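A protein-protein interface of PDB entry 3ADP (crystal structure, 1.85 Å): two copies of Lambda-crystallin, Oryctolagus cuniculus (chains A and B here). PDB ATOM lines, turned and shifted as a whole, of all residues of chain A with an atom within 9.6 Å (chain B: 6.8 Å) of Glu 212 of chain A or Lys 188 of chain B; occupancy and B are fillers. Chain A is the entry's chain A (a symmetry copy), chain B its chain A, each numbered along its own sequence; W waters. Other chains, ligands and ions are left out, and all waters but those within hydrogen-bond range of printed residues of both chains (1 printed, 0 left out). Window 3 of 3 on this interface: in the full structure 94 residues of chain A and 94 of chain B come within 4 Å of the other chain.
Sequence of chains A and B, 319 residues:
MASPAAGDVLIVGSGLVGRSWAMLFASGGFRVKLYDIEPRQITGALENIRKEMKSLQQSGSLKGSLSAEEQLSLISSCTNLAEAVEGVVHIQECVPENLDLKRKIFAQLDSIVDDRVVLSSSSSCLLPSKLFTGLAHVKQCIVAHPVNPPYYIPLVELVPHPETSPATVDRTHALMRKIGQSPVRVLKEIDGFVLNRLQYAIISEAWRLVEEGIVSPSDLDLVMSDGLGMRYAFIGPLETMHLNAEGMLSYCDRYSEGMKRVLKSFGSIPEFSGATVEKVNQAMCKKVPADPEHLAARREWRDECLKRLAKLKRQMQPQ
N of Leu 187 of chain B lies within hydrogen-bond range of O of Ile 214 of chain A, at 2.8 Å. The backbone carbonyl oxygen (O) of Glu 212 of chain A is in hydrogen-bond range of the side-chain amino group (NZ) of Lys 188 of chain B (2.9 Å).
O of Leu 158 of chain B is in hydrogen-bond range of N of Val 186 of chain B (3.0 Å). N of Ile 214 of chain A sits at hydrogen-bond distance from O of Leu 209 of chain A, 2.9 Å away.
Among the printed residues, pairs that only touch across the chains: Gly 213 of chain A with Leu 187 of chain B (3.2 Å), Ile 214 of chain A with Val 186 of chain B (3.4 Å), Gly 213 of chain A with Lys 188 of chain B (3.6 Å), Ile 214 of chain A with Ile 190 of chain B (3.8 Å), Val 215 of chain A with Arg 185 of chain B (3.8 Å), Ile 214 of chain A with Arg 185 of chain B (3.96 Å) and Ile 214 of chain A with Lys 188 of chain B (3.98 Å).
Of chain B, only Lys 188 (2.9 Å) comes within 4 Å of Glu 212 of chain A. Of the printed residues of chain A, Lys 188 of chain B touches Glu 212 (2.9 Å), Gly 213 (3.6 Å) and Ile 214 (3.98 Å). Printed residues of chain B within 4 Å of Ile 214 of chain A: Arg 185 (3.96 Å), Val 186 (3.4 Å), Leu 187 (2.8 Å), Lys 188 (3.98 Å) and Ile 190 (3.8 Å). Printed residues of chain A within 4 Å of Ile 190 of chain B: Ile 214. Of the printed residues of chain A, Arg 185 of chain B touches Ile 214 and Val 215. Printed residues of chain B within 4 Å of Val 215 of chain A: Arg 185. The nearest residue of chain B that does not touch Glu 212 of chain A is Ile 190 of chain B (6.4 Å). The nearest printed residue of chain A that does not touch Arg 185 of chain B is Ser 216 of chain A (4.8 Å).
Of the 10 printed residues of chain B, 5 touch a printed residue of chain A. Hydrophobic or aromatic side chains of chain B that line the printed part of chain A: Val 186, Leu 187 and Ile 190. Of the 22 printed residues of chain A, 4 touch a printed residue of chain B. Among the printed residues, 9 pairs touch across the chains. Among the printed residues, no Asp or Glu carboxylate lies within 4 Å of a Lys or Arg side-chain nitrogen of the other chain.
No position is printed for both chains. Of the 9 pairs that touch across the chains among the printed residues, none has its exchanged pair printed and touching as well.
Water W1 bridges the backbone carbonyl oxygen of Arg 185 of chain B (2.7 Å) and the backbone NH of Ser 216 of chain A (3.1 Å).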
ATOM      1  N   SER A 204      22.314 -11.632  17.613  1.00  0.00           N
ATOM      2  CA  SER A 204      21.748 -10.948  16.456  1.00  0.00           C
ATOM      3  C   SER A 204      20.219 -10.868  16.519  1.00  0.00           C
ATOM      4  O   SER A 204      19.640  -9.799  16.341  1.00  0.00           O
ATOM      5  CB  SER A 204      22.177 -11.659  15.168  1.00  0.00           C
ATOM      6  OG  SER A 204      21.800 -10.912  14.023  1.00  0.00           O
ATOM      7  N   GLU A 205      19.570 -11.998  16.778  1.00  0.00           N
ATOM      8  CA  GLU A 205      18.109 -12.029  16.862  1.00  0.00           C
ATOM      9  C   GLU A 205      17.630 -11.291  18.111  1.00  0.00           C
ATOM     10  O   GLU A 205      16.651 -10.546  18.057  1.00  0.00           O
ATOM     11  CB  GLU A 205      17.613 -13.482  16.860  1.00  0.00           C
ATOM     12  CG  GLU A 205      16.116 -13.677  17.134  1.00  0.00           C
ATOM     13  CD  GLU A 205      15.213 -12.905  16.187  1.00  0.00           C
ATOM     14  OE1 GLU A 205      15.687 -12.467  15.117  1.00  0.00           O
ATOM     15  OE2 GLU A 205      14.014 -12.749  16.510  1.00  0.00           O
ATOM     16  N   ALA A 206      18.321 -11.485  19.231  1.00  0.00           N
ATOM     17  CA  ALA A 206      17.943 -10.809  20.468  1.00  0.00           C
ATOM     18  C   ALA A 206      17.968  -9.293  20.271  1.00  0.00           C
ATOM     19  O   ALA A 206      17.062  -8.580  20.711  1.00  0.00           O
ATOM     20  CB  ALA A 206      18.897 -11.200  21.596  1.00  0.00           C
ATOM     21  N   TRP A 207      19.011  -8.813  19.601  1.00  0.00           N
ATOM     22  CA  TRP A 207      19.182  -7.388  19.345  1.00  0.00           C
ATOM     23  C   TRP A 207      18.007  -6.812  18.562  1.00  0.00           C
ATOM     24  O   TRP A 207      17.490  -5.747  18.901  1.00  0.00           O
ATOM     25  CB  TRP A 207      20.495  -7.154  18.593  1.00  0.00           C
ATOM     26  CG  TRP A 207      21.043  -5.773  18.739  1.00  0.00           C
ATOM     27  CD1 TRP A 207      20.828  -4.709  17.912  1.00  0.00           C
ATOM     28  CD2 TRP A 207      21.899  -5.302  19.787  1.00  0.00           C
ATOM     29  NE1 TRP A 207      21.502  -3.602  18.379  1.00  0.00           N
ATOM     30  CE2 TRP A 207      22.165  -3.940  19.530  1.00  0.00           C
ATOM     31  CE3 TRP A 207      22.467  -5.901  20.921  1.00  0.00           C
ATOM     32  CZ2 TRP A 207      22.978  -3.163  20.365  1.00  0.00           C
ATOM     33  CZ3 TRP A 207      23.277  -5.129  21.752  1.00  0.00           C
ATOM     34  CH2 TRP A 207      23.523  -3.772  21.467  1.00  0.00           C
ATOM     35  N   ARG A 208      17.579  -7.518  17.519  1.00  0.00           N
ATOM     36  CA  ARG A 208      16.453  -7.062  16.710  1.00  0.00           C
ATOM     37  C   ARG A 208      15.136  -7.107  17.490  1.00  0.00           C
ATOM     38  O   ARG A 208      14.273  -6.256  17.296  1.00  0.00           O
ATOM     39  CB  ARG A 208      16.328  -7.900  15.433  1.00  0.00           C
ATOM     40  CG  ARG A 208      17.395  -7.606  14.378  1.00  0.00           C
ATOM     41  CD  ARG A 208      17.071  -8.312  13.071  1.00  0.00           C
ATOM     42  NE  ARG A 208      17.055  -9.763  13.232  1.00  0.00           N
ATOM     43  CZ  ARG A 208      18.128 -10.542  13.132  1.00  0.00           C
ATOM     44  NH1 ARG A 208      19.314 -10.019  12.859  1.00  0.00           N
ATOM     45  NH2 ARG A 208      18.019 -11.849  13.324  1.00  0.00           N
ATOM     46  N   LEU A 209      14.981  -8.094  18.368  1.00  0.00           N
ATOM     47  CA  LEU A 209      13.758  -8.200  19.160  1.00  0.00           C
ATOM     48  C   LEU A 209      13.621  -6.997  20.092  1.00  0.00           C
ATOM     49  O   LEU A 209      12.519  -6.484  20.300  1.00  0.00           O
ATOM     50  CB  LEU A 209      13.751  -9.507  19.966  1.00  0.00           C
ATOM     51  CG  LEU A 209      13.580 -10.782  19.133  1.00  0.00           C
ATOM     52  CD1 LEU A 209      13.731 -12.020  20.009  1.00  0.00           C
ATOM     53  CD2 LEU A 209      12.209 -10.759  18.465  1.00  0.00           C
ATOM     54  N   VAL A 210      14.741  -6.547  20.651  1.00  0.00           N
ATOM     55  CA  VAL A 210      14.732  -5.389  21.537  1.00  0.00           C
ATOM     56  C   VAL A 210      14.501  -4.131  20.705  1.00  0.00           C
ATOM     57  O   VAL A 210      13.704  -3.268  21.075  1.00  0.00           O
ATOM     58  CB  VAL A 210      16.075  -5.232  22.294  1.00  0.00           C
ATOM     59  CG1 VAL A 210      16.107  -3.897  23.027  1.00  0.00           C
ATOM     60  CG2 VAL A 210      16.258  -6.373  23.278  1.00  0.00           C
ATOM     61  N   GLU A 211      15.202  -4.036  19.579  1.00  0.00           N
ATOM     62  CA  GLU A 211      15.072  -2.886  18.693  1.00  0.00           C
ATOM     63  C   GLU A 211      13.643  -2.708  18.181  1.00  0.00           C
ATOM     64  O   GLU A 211      13.162  -1.582  18.059  1.00  0.00           O
ATOM     65  CB  GLU A 211      16.023  -3.020  17.499  1.00  0.00           C
ATOM     66  CG  GLU A 211      15.926  -1.864  16.508  1.00  0.00           C
ATOM     67  CD  GLU A 211      16.897  -1.994  15.347  1.00  0.00           C
ATOM     68  OE1 GLU A 211      16.814  -2.994  14.603  1.00  0.00           O
ATOM     69  OE2 GLU A 211      17.742  -1.092  15.177  1.00  0.00           O
ATOM     70  N   GLU A 212      12.967  -3.815  17.885  1.00  0.00           N
ATOM     71  CA  GLU A 212      11.597  -3.754  17.374  1.00  0.00           C
ATOM     72  C   GLU A 212      10.523  -3.636  18.454  1.00  0.00           C
ATOM     73  O   GLU A 212       9.329  -3.629  18.148  1.00  0.00           O
ATOM     74  CB  GLU A 212      11.305  -4.974  16.494  1.00  0.00           C
ATOM     75  CG  GLU A 212      12.089  -4.999  15.190  1.00  0.00           C
ATOM     76  CD  GLU A 212      11.881  -3.743  14.359  1.00  0.00           C
ATOM     77  OE1 GLU A 212      10.711  -3.358  14.139  1.00  0.00           O
ATOM     78  OE2 GLU A 212      12.887  -3.144  13.923  1.00  0.00           O
ATOM     79  N   GLY A 213      10.950  -3.549  19.710  1.00  0.00           N
ATOM     80  CA  GLY A 213      10.008  -3.414  20.807  1.00  0.00           C
ATOM     81  C   GLY A 213       9.191  -4.649  21.138  1.00  0.00           C
ATOM     82  O   GLY A 213       8.072  -4.539  21.642  1.00  0.00           O
ATOM     83  N   ILE A 214       9.739  -5.824  20.855  1.00  0.00           N
ATOM     84  CA  ILE A 214       9.044  -7.073  21.150  1.00  0.00           C
ATOM     85  C   ILE A 214       9.166  -7.396  22.636  1.00  0.00           C
ATOM     86  O   ILE A 214       8.228  -7.910  23.255  1.00  0.00           O
ATOM     87  CB  ILE A 214       9.638  -8.248  20.342  1.00  0.00           C
ATOM     88  CG1 ILE A 214       9.544  -7.948  18.844  1.00  0.00           C
ATOM     89  CG2 ILE A 214       8.920  -9.547  20.701  1.00  0.00           C
ATOM     90  CD1 ILE A 214       8.139  -7.641  18.354  1.00  0.00           C
ATOM     91  N   VAL A 215      10.321  -7.080  23.210  1.00  0.00           N
ATOM     92  CA  VAL A 215      10.566  -7.356  24.619  1.00  0.00           C
ATOM     93  C   VAL A 215      11.687  -6.462  25.142  1.00  0.00           C
ATOM     94  O   VAL A 215      12.554  -6.034  24.381  1.00  0.00           O
ATOM     95  CB  VAL A 215      10.941  -8.853  24.817  1.00  0.00           C
ATOM     96  CG1 VAL A 215      12.235  -9.175  24.079  1.00  0.00           C
ATOM     97  CG2 VAL A 215      11.062  -9.174  26.284  1.00  0.00           C
ATOM     98  N   SER A 216      11.657  -6.165  26.437  1.00  0.00           N
ATOM     99  CA  SER A 216      12.684  -5.321  27.039  1.00  0.00           C
ATOM    100  C   SER A 216      13.975  -6.132  27.125  1.00  0.00           C
ATOM    101  O   SER A 216      13.946  -7.362  27.087  1.00  0.00           O
ATOM    102  CB  SER A 216      12.260  -4.881  28.442  1.00  0.00           C
ATOM    103  OG  SER A 216      12.345  -5.958  29.364  1.00  0.00           O
ATOM    104  N   PRO A 217      15.128  -5.454  27.231  1.00  0.00           N
ATOM    105  CA  PRO A 217      16.410  -6.160  27.320  1.00  0.00           C
ATOM    106  C   PRO A 217      16.460  -7.129  28.500  1.00  0.00           C
ATOM    107  O   PRO A 217      16.931  -8.262  28.372  1.00  0.00           O
ATOM    108  CB  PRO A 217      17.417  -5.023  27.465  1.00  0.00           C
ATOM    109  CG  PRO A 217      16.774  -3.913  26.659  1.00  0.00           C
ATOM    110  CD  PRO A 217      15.334  -3.997  27.108  1.00  0.00           C
ATOM    111  N   LEU A 220      14.228 -10.120  27.865  1.00  0.00           N
ATOM    112  CA  LEU A 220      14.802 -11.022  26.875  1.00  0.00           C
ATOM    113  C   LEU A 220      15.814 -11.921  27.573  1.00  0.00           C
ATOM    114  O   LEU A 220      15.838 -13.131  27.342  1.00  0.00           O
ATOM    115  CB  LEU A 220      15.483 -10.258  25.734  1.00  0.00           C
ATOM    116  CG  LEU A 220      16.027 -11.206  24.654  1.00  0.00           C
ATOM    117  CD1 LEU A 220      15.801 -10.620  23.277  1.00  0.00           C
ATOM    118  CD2 LEU A 220      17.501 -11.487  24.905  1.00  0.00           C
ATOM    119  N   SER A 265      11.419 -14.444   8.545  1.00  0.00           N
ATOM    120  CA  SER A 265      11.015 -13.125   9.028  1.00  0.00           C
ATOM    121  C   SER A 265      12.133 -12.352   9.726  1.00  0.00           C
ATOM    122  O   SER A 265      11.951 -11.191  10.083  1.00  0.00           O
ATOM    123  CB  SER A 265       9.817 -13.250   9.981  1.00  0.00           C
ATOM    124  OG  SER A 265      10.211 -13.760  11.247  1.00  0.00           O
ATOM    125  N   PHE A 266      13.286 -12.988   9.918  1.00  0.00           N
ATOM    126  CA  PHE A 266      14.419 -12.332  10.573  1.00  0.00           C
ATOM    127  C   PHE A 266      14.887 -11.094   9.814  1.00  0.00           C
ATOM    128  O   PHE A 266      15.010 -11.116   8.588  1.00  0.00           O
ATOM    129  CB  PHE A 266      15.590 -13.309  10.709  1.00  0.00           C
ATOM    130  CG  PHE A 266      15.526 -14.175  11.940  1.00  0.00           C
ATOM    131  CD1 PHE A 266      14.307 -14.490  12.533  1.00  0.00           C
ATOM    132  CD2 PHE A 266      16.692 -14.694  12.493  1.00  0.00           C
ATOM    133  CE1 PHE A 266      14.249 -15.312  13.661  1.00  0.00           C
ATOM    134  CE2 PHE A 266      16.646 -15.518  13.623  1.00  0.00           C
ATOM    135  CZ  PHE A 266      15.421 -15.826  14.207  1.00  0.00           C
ATOM    136  N   GLY A 267      15.150 -10.022  10.555  1.00  0.00           N
ATOM    137  CA  GLY A 267      15.613  -8.785   9.954  1.00  0.00           C
ATOM    138  C   GLY A 267      17.075  -8.834   9.537  1.00  0.00           C
ATOM    139  O   GLY A 267      17.679  -9.903   9.476  1.00  0.00           O
ATOM    140  N   SER A 268      17.652  -7.668   9.263  1.00  0.00           N
ATOM    141  CA  SER A 268      19.044  -7.586   8.827  1.00  0.00           C
ATOM    142  C   SER A 268      20.057  -7.632   9.968  1.00  0.00           C
ATOM    143  O   SER A 268      19.695  -7.591  11.143  1.00  0.00           O
ATOM    144  CB  SER A 268      19.254  -6.305   8.011  1.00  0.00           C
ATOM    145  OG  SER A 268      18.896  -5.164   8.772  1.00  0.00           O
ATOM    146  N   THR A 276      19.699   1.601  19.764  1.00  0.00           N
ATOM    147  CA  THR A 276      19.593   0.296  20.408  1.00  0.00           C
ATOM    148  C   THR A 276      20.720  -0.008  21.392  1.00  0.00           C
ATOM    149  O   THR A 276      20.477  -0.597  22.446  1.00  0.00           O
ATOM    150  CB  THR A 276      19.500  -0.834  19.365  1.00  0.00           C
ATOM    151  OG1 THR A 276      18.410  -0.567  18.472  1.00  0.00           O
ATOM    152  CG2 THR A 276      19.245  -2.170  20.053  1.00  0.00           C
ATOM    153  N   LYS A 279      19.844   1.873  24.431  1.00  0.00           N
ATOM    154  CA  LYS A 279      18.729   1.241  25.128  1.00  0.00           C
ATOM    155  C   LYS A 279      19.171  -0.016  25.877  1.00  0.00           C
ATOM    156  O   LYS A 279      18.835  -0.207  27.046  1.00  0.00           O
ATOM    157  CB  LYS A 279      17.630   0.883  24.129  1.00  0.00           C
ATOM    158  CG  LYS A 279      16.376   0.314  24.763  1.00  0.00           C
ATOM    159  CD  LYS A 279      15.282   0.164  23.723  1.00  0.00           C
ATOM    160  CE  LYS A 279      13.961  -0.226  24.355  1.00  0.00           C
ATOM    161  NZ  LYS A 279      12.888  -0.276  23.330  1.00  0.00           N
ATOM    162  N   VAL A 280      19.921  -0.877  25.199  1.00  0.00           N
ATOM    163  CA  VAL A 280      20.400  -2.100  25.827  1.00  0.00           C
ATOM    164  C   VAL A 280      21.355  -1.776  26.972  1.00  0.00           C
ATOM    165  O   VAL A 280      21.213  -2.305  28.073  1.00  0.00           O
ATOM    166  CB  VAL A 280      21.115  -3.016  24.805  1.00  0.00           C
ATOM    167  CG1 VAL A 280      21.751  -4.195  25.516  1.00  0.00           C
ATOM    168  CG2 VAL A 280      20.112  -3.511  23.770  1.00  0.00           C
ATOM    169  N   LEU B 158       4.203 -13.921  28.512  1.00  0.00           N
ATOM    170  CA  LEU B 158       2.910 -13.256  28.501  1.00  0.00           C
ATOM    171  C   LEU B 158       2.805 -12.511  27.183  1.00  0.00           C
ATOM    172  O   LEU B 158       3.507 -11.524  26.959  1.00  0.00           O
ATOM    173  CB  LEU B 158       2.795 -12.269  29.666  1.00  0.00           C
ATOM    174  CG  LEU B 158       2.996 -12.860  31.062  1.00  0.00           C
ATOM    175  CD1 LEU B 158       2.832 -11.766  32.106  1.00  0.00           C
ATOM    176  CD2 LEU B 158       1.987 -13.980  31.294  1.00  0.00           C
ATOM    177  N   VAL B 159       1.936 -12.998  26.306  1.00  0.00           N
ATOM    178  CA  VAL B 159       1.743 -12.384  25.003  1.00  0.00           C
ATOM    179  C   VAL B 159       0.316 -11.853  24.932  1.00  0.00           C
ATOM    180  O   VAL B 159      -0.652 -12.614  24.986  1.00  0.00           O
ATOM    181  CB  VAL B 159       1.967 -13.405  23.872  1.00  0.00           C
ATOM    182  CG1 VAL B 159       2.147 -12.681  22.547  1.00  0.00           C
ATOM    183  CG2 VAL B 159       3.185 -14.268  24.191  1.00  0.00           C
ATOM    184  N   PRO B 160       0.172 -10.528  24.815  1.00  0.00           N
ATOM    185  CA  PRO B 160      -1.133  -9.871  24.744  1.00  0.00           C
ATOM    186  C   PRO B 160      -1.740  -9.718  23.358  1.00  0.00           C
ATOM    187  O   PRO B 160      -1.053  -9.807  22.339  1.00  0.00           O
ATOM    188  CB  PRO B 160      -0.847  -8.511  25.356  1.00  0.00           C
ATOM    189  CG  PRO B 160       0.505  -8.206  24.759  1.00  0.00           C
ATOM    190  CD  PRO B 160       1.253  -9.529  24.917  1.00  0.00           C
ATOM    191  N   ARG B 185       7.164  -9.837  29.758  1.00  0.00           N
ATOM    192  CA  ARG B 185       6.175  -9.130  28.963  1.00  0.00           C
ATOM    193  C   ARG B 185       6.554  -9.042  27.491  1.00  0.00           C
ATOM    194  O   ARG B 185       7.422  -8.253  27.118  1.00  0.00           O
ATOM    195  CB  ARG B 185       5.977  -7.706  29.492  1.00  0.00           C
ATOM    196  CG  ARG B 185       5.297  -7.593  30.849  1.00  0.00           C
ATOM    197  CD  ARG B 185       4.975  -6.131  31.134  1.00  0.00           C
ATOM    198  NE  ARG B 185       4.168  -5.942  32.336  1.00  0.00           N
ATOM    199  CZ  ARG B 185       4.624  -6.056  33.578  1.00  0.00           C
ATOM    200  NH1 ARG B 185       5.897  -6.360  33.795  1.00  0.00           N
ATOM    201  NH2 ARG B 185       3.805  -5.865  34.604  1.00  0.00           N
ATOM    202  N   VAL B 186       5.928  -9.865  26.655  1.00  0.00           N
ATOM    203  CA  VAL B 186       6.183  -9.783  25.226  1.00  0.00           C
ATOM    204  C   VAL B 186       5.252  -8.633  24.844  1.00  0.00           C
ATOM    205  O   VAL B 186       4.036  -8.795  24.812  1.00  0.00           O
ATOM    206  CB  VAL B 186       5.775 -11.078  24.489  1.00  0.00           C
ATOM    207  CG1 VAL B 186       6.112 -10.958  23.016  1.00  0.00           C
ATOM    208  CG2 VAL B 186       6.502 -12.272  25.096  1.00  0.00           C
ATOM    209  N   LEU B 187       5.839  -7.471  24.585  1.00  0.00           N
ATOM    210  CA  LEU B 187       5.093  -6.255  24.278  1.00  0.00           C
ATOM    211  C   LEU B 187       4.152  -6.288  23.086  1.00  0.00           C
ATOM    212  O   LEU B 187       3.091  -5.665  23.117  1.00  0.00           O
ATOM    213  CB  LEU B 187       6.078  -5.095  24.117  1.00  0.00           C
ATOM    214  CG  LEU B 187       6.995  -4.937  25.330  1.00  0.00           C
ATOM    215  CD1 LEU B 187       8.002  -3.825  25.083  1.00  0.00           C
ATOM    216  CD2 LEU B 187       6.152  -4.655  26.564  1.00  0.00           C
ATOM    217  N   LYS B 188       4.548  -7.001  22.039  1.00  0.00           N
ATOM    218  CA  LYS B 188       3.735  -7.116  20.834  1.00  0.00           C
ATOM    219  C   LYS B 188       3.835  -8.557  20.350  1.00  0.00           C
ATOM    220  O   LYS B 188       4.918  -9.139  20.359  1.00  0.00           O
ATOM    221  CB  LYS B 188       4.254  -6.158  19.757  1.00  0.00           C
ATOM    222  CG  LYS B 188       4.223  -4.691  20.179  1.00  0.00           C
ATOM    223  CD  LYS B 188       4.670  -3.757  19.058  1.00  0.00           C
ATOM    224  CE  LYS B 188       6.125  -3.976  18.681  1.00  0.00           C
ATOM    225  NZ  LYS B 188       6.571  -3.018  17.622  1.00  0.00           N
ATOM    226  N   GLU B 189       2.713  -9.139  19.939  1.00  0.00           N
ATOM    227  CA  GLU B 189       2.744 -10.517  19.478  1.00  0.00           C
ATOM    228  C   GLU B 189       3.653 -10.667  18.272  1.00  0.00           C
ATOM    229  O   GLU B 189       3.820  -9.739  17.477  1.00  0.00           O
ATOM    230  CB  GLU B 189       1.344 -11.012  19.112  1.00  0.00           C
ATOM    231  CG  GLU B 189       0.666 -10.216  18.005  1.00  0.00           C
ATOM    232  CD  GLU B 189      -0.634 -10.850  17.562  1.00  0.00           C
ATOM    233  OE1 GLU B 189      -1.323 -11.438  18.419  1.00  0.00           O
ATOM    234  OE2 GLU B 189      -0.973 -10.751  16.362  1.00  0.00           O
ATOM    235  N   ILE B 190       4.252 -11.843  18.152  1.00  0.00           N
ATOM    236  CA  ILE B 190       5.127 -12.135  17.030  1.00  0.00           C
ATOM    237  C   ILE B 190       5.246 -13.648  16.901  1.00  0.00           C
ATOM    238  O   ILE B 190       5.194 -14.376  17.891  1.00  0.00           O
ATOM    239  CB  ILE B 190       6.529 -11.485  17.211  1.00  0.00           C
ATOM    240  CG1 ILE B 190       7.338 -11.628  15.919  1.00  0.00           C
ATOM    241  CG2 ILE B 190       7.269 -12.127  18.382  1.00  0.00           C
ATOM    242  CD1 ILE B 190       8.608 -10.789  15.886  1.00  0.00           C
ATOM    243  N   PHE B 193       6.962 -16.020  19.339  1.00  0.00           N
ATOM    244  CA  PHE B 193       7.133 -15.229  20.557  1.00  0.00           C
ATOM    245  C   PHE B 193       8.613 -14.882  20.709  1.00  0.00           C
ATOM    246  O   PHE B 193       9.216 -14.376  19.765  1.00  0.00           O
ATOM    247  CB  PHE B 193       6.605 -15.995  21.781  1.00  0.00           C
ATOM    248  CG  PHE B 193       5.163 -16.428  21.651  1.00  0.00           C
ATOM    249  CD1 PHE B 193       4.255 -15.671  20.910  1.00  0.00           C
ATOM    250  CD2 PHE B 193       4.713 -17.593  22.265  1.00  0.00           C
ATOM    251  CE1 PHE B 193       2.919 -16.071  20.782  1.00  0.00           C
ATOM    252  CE2 PHE B 193       3.380 -18.003  22.145  1.00  0.00           C
ATOM    253  CZ  PHE B 193       2.483 -17.241  21.400  1.00  0.00           C
HETATM  254  O   HOH W   1       9.248  -6.691  28.333  1.00  0.00           O
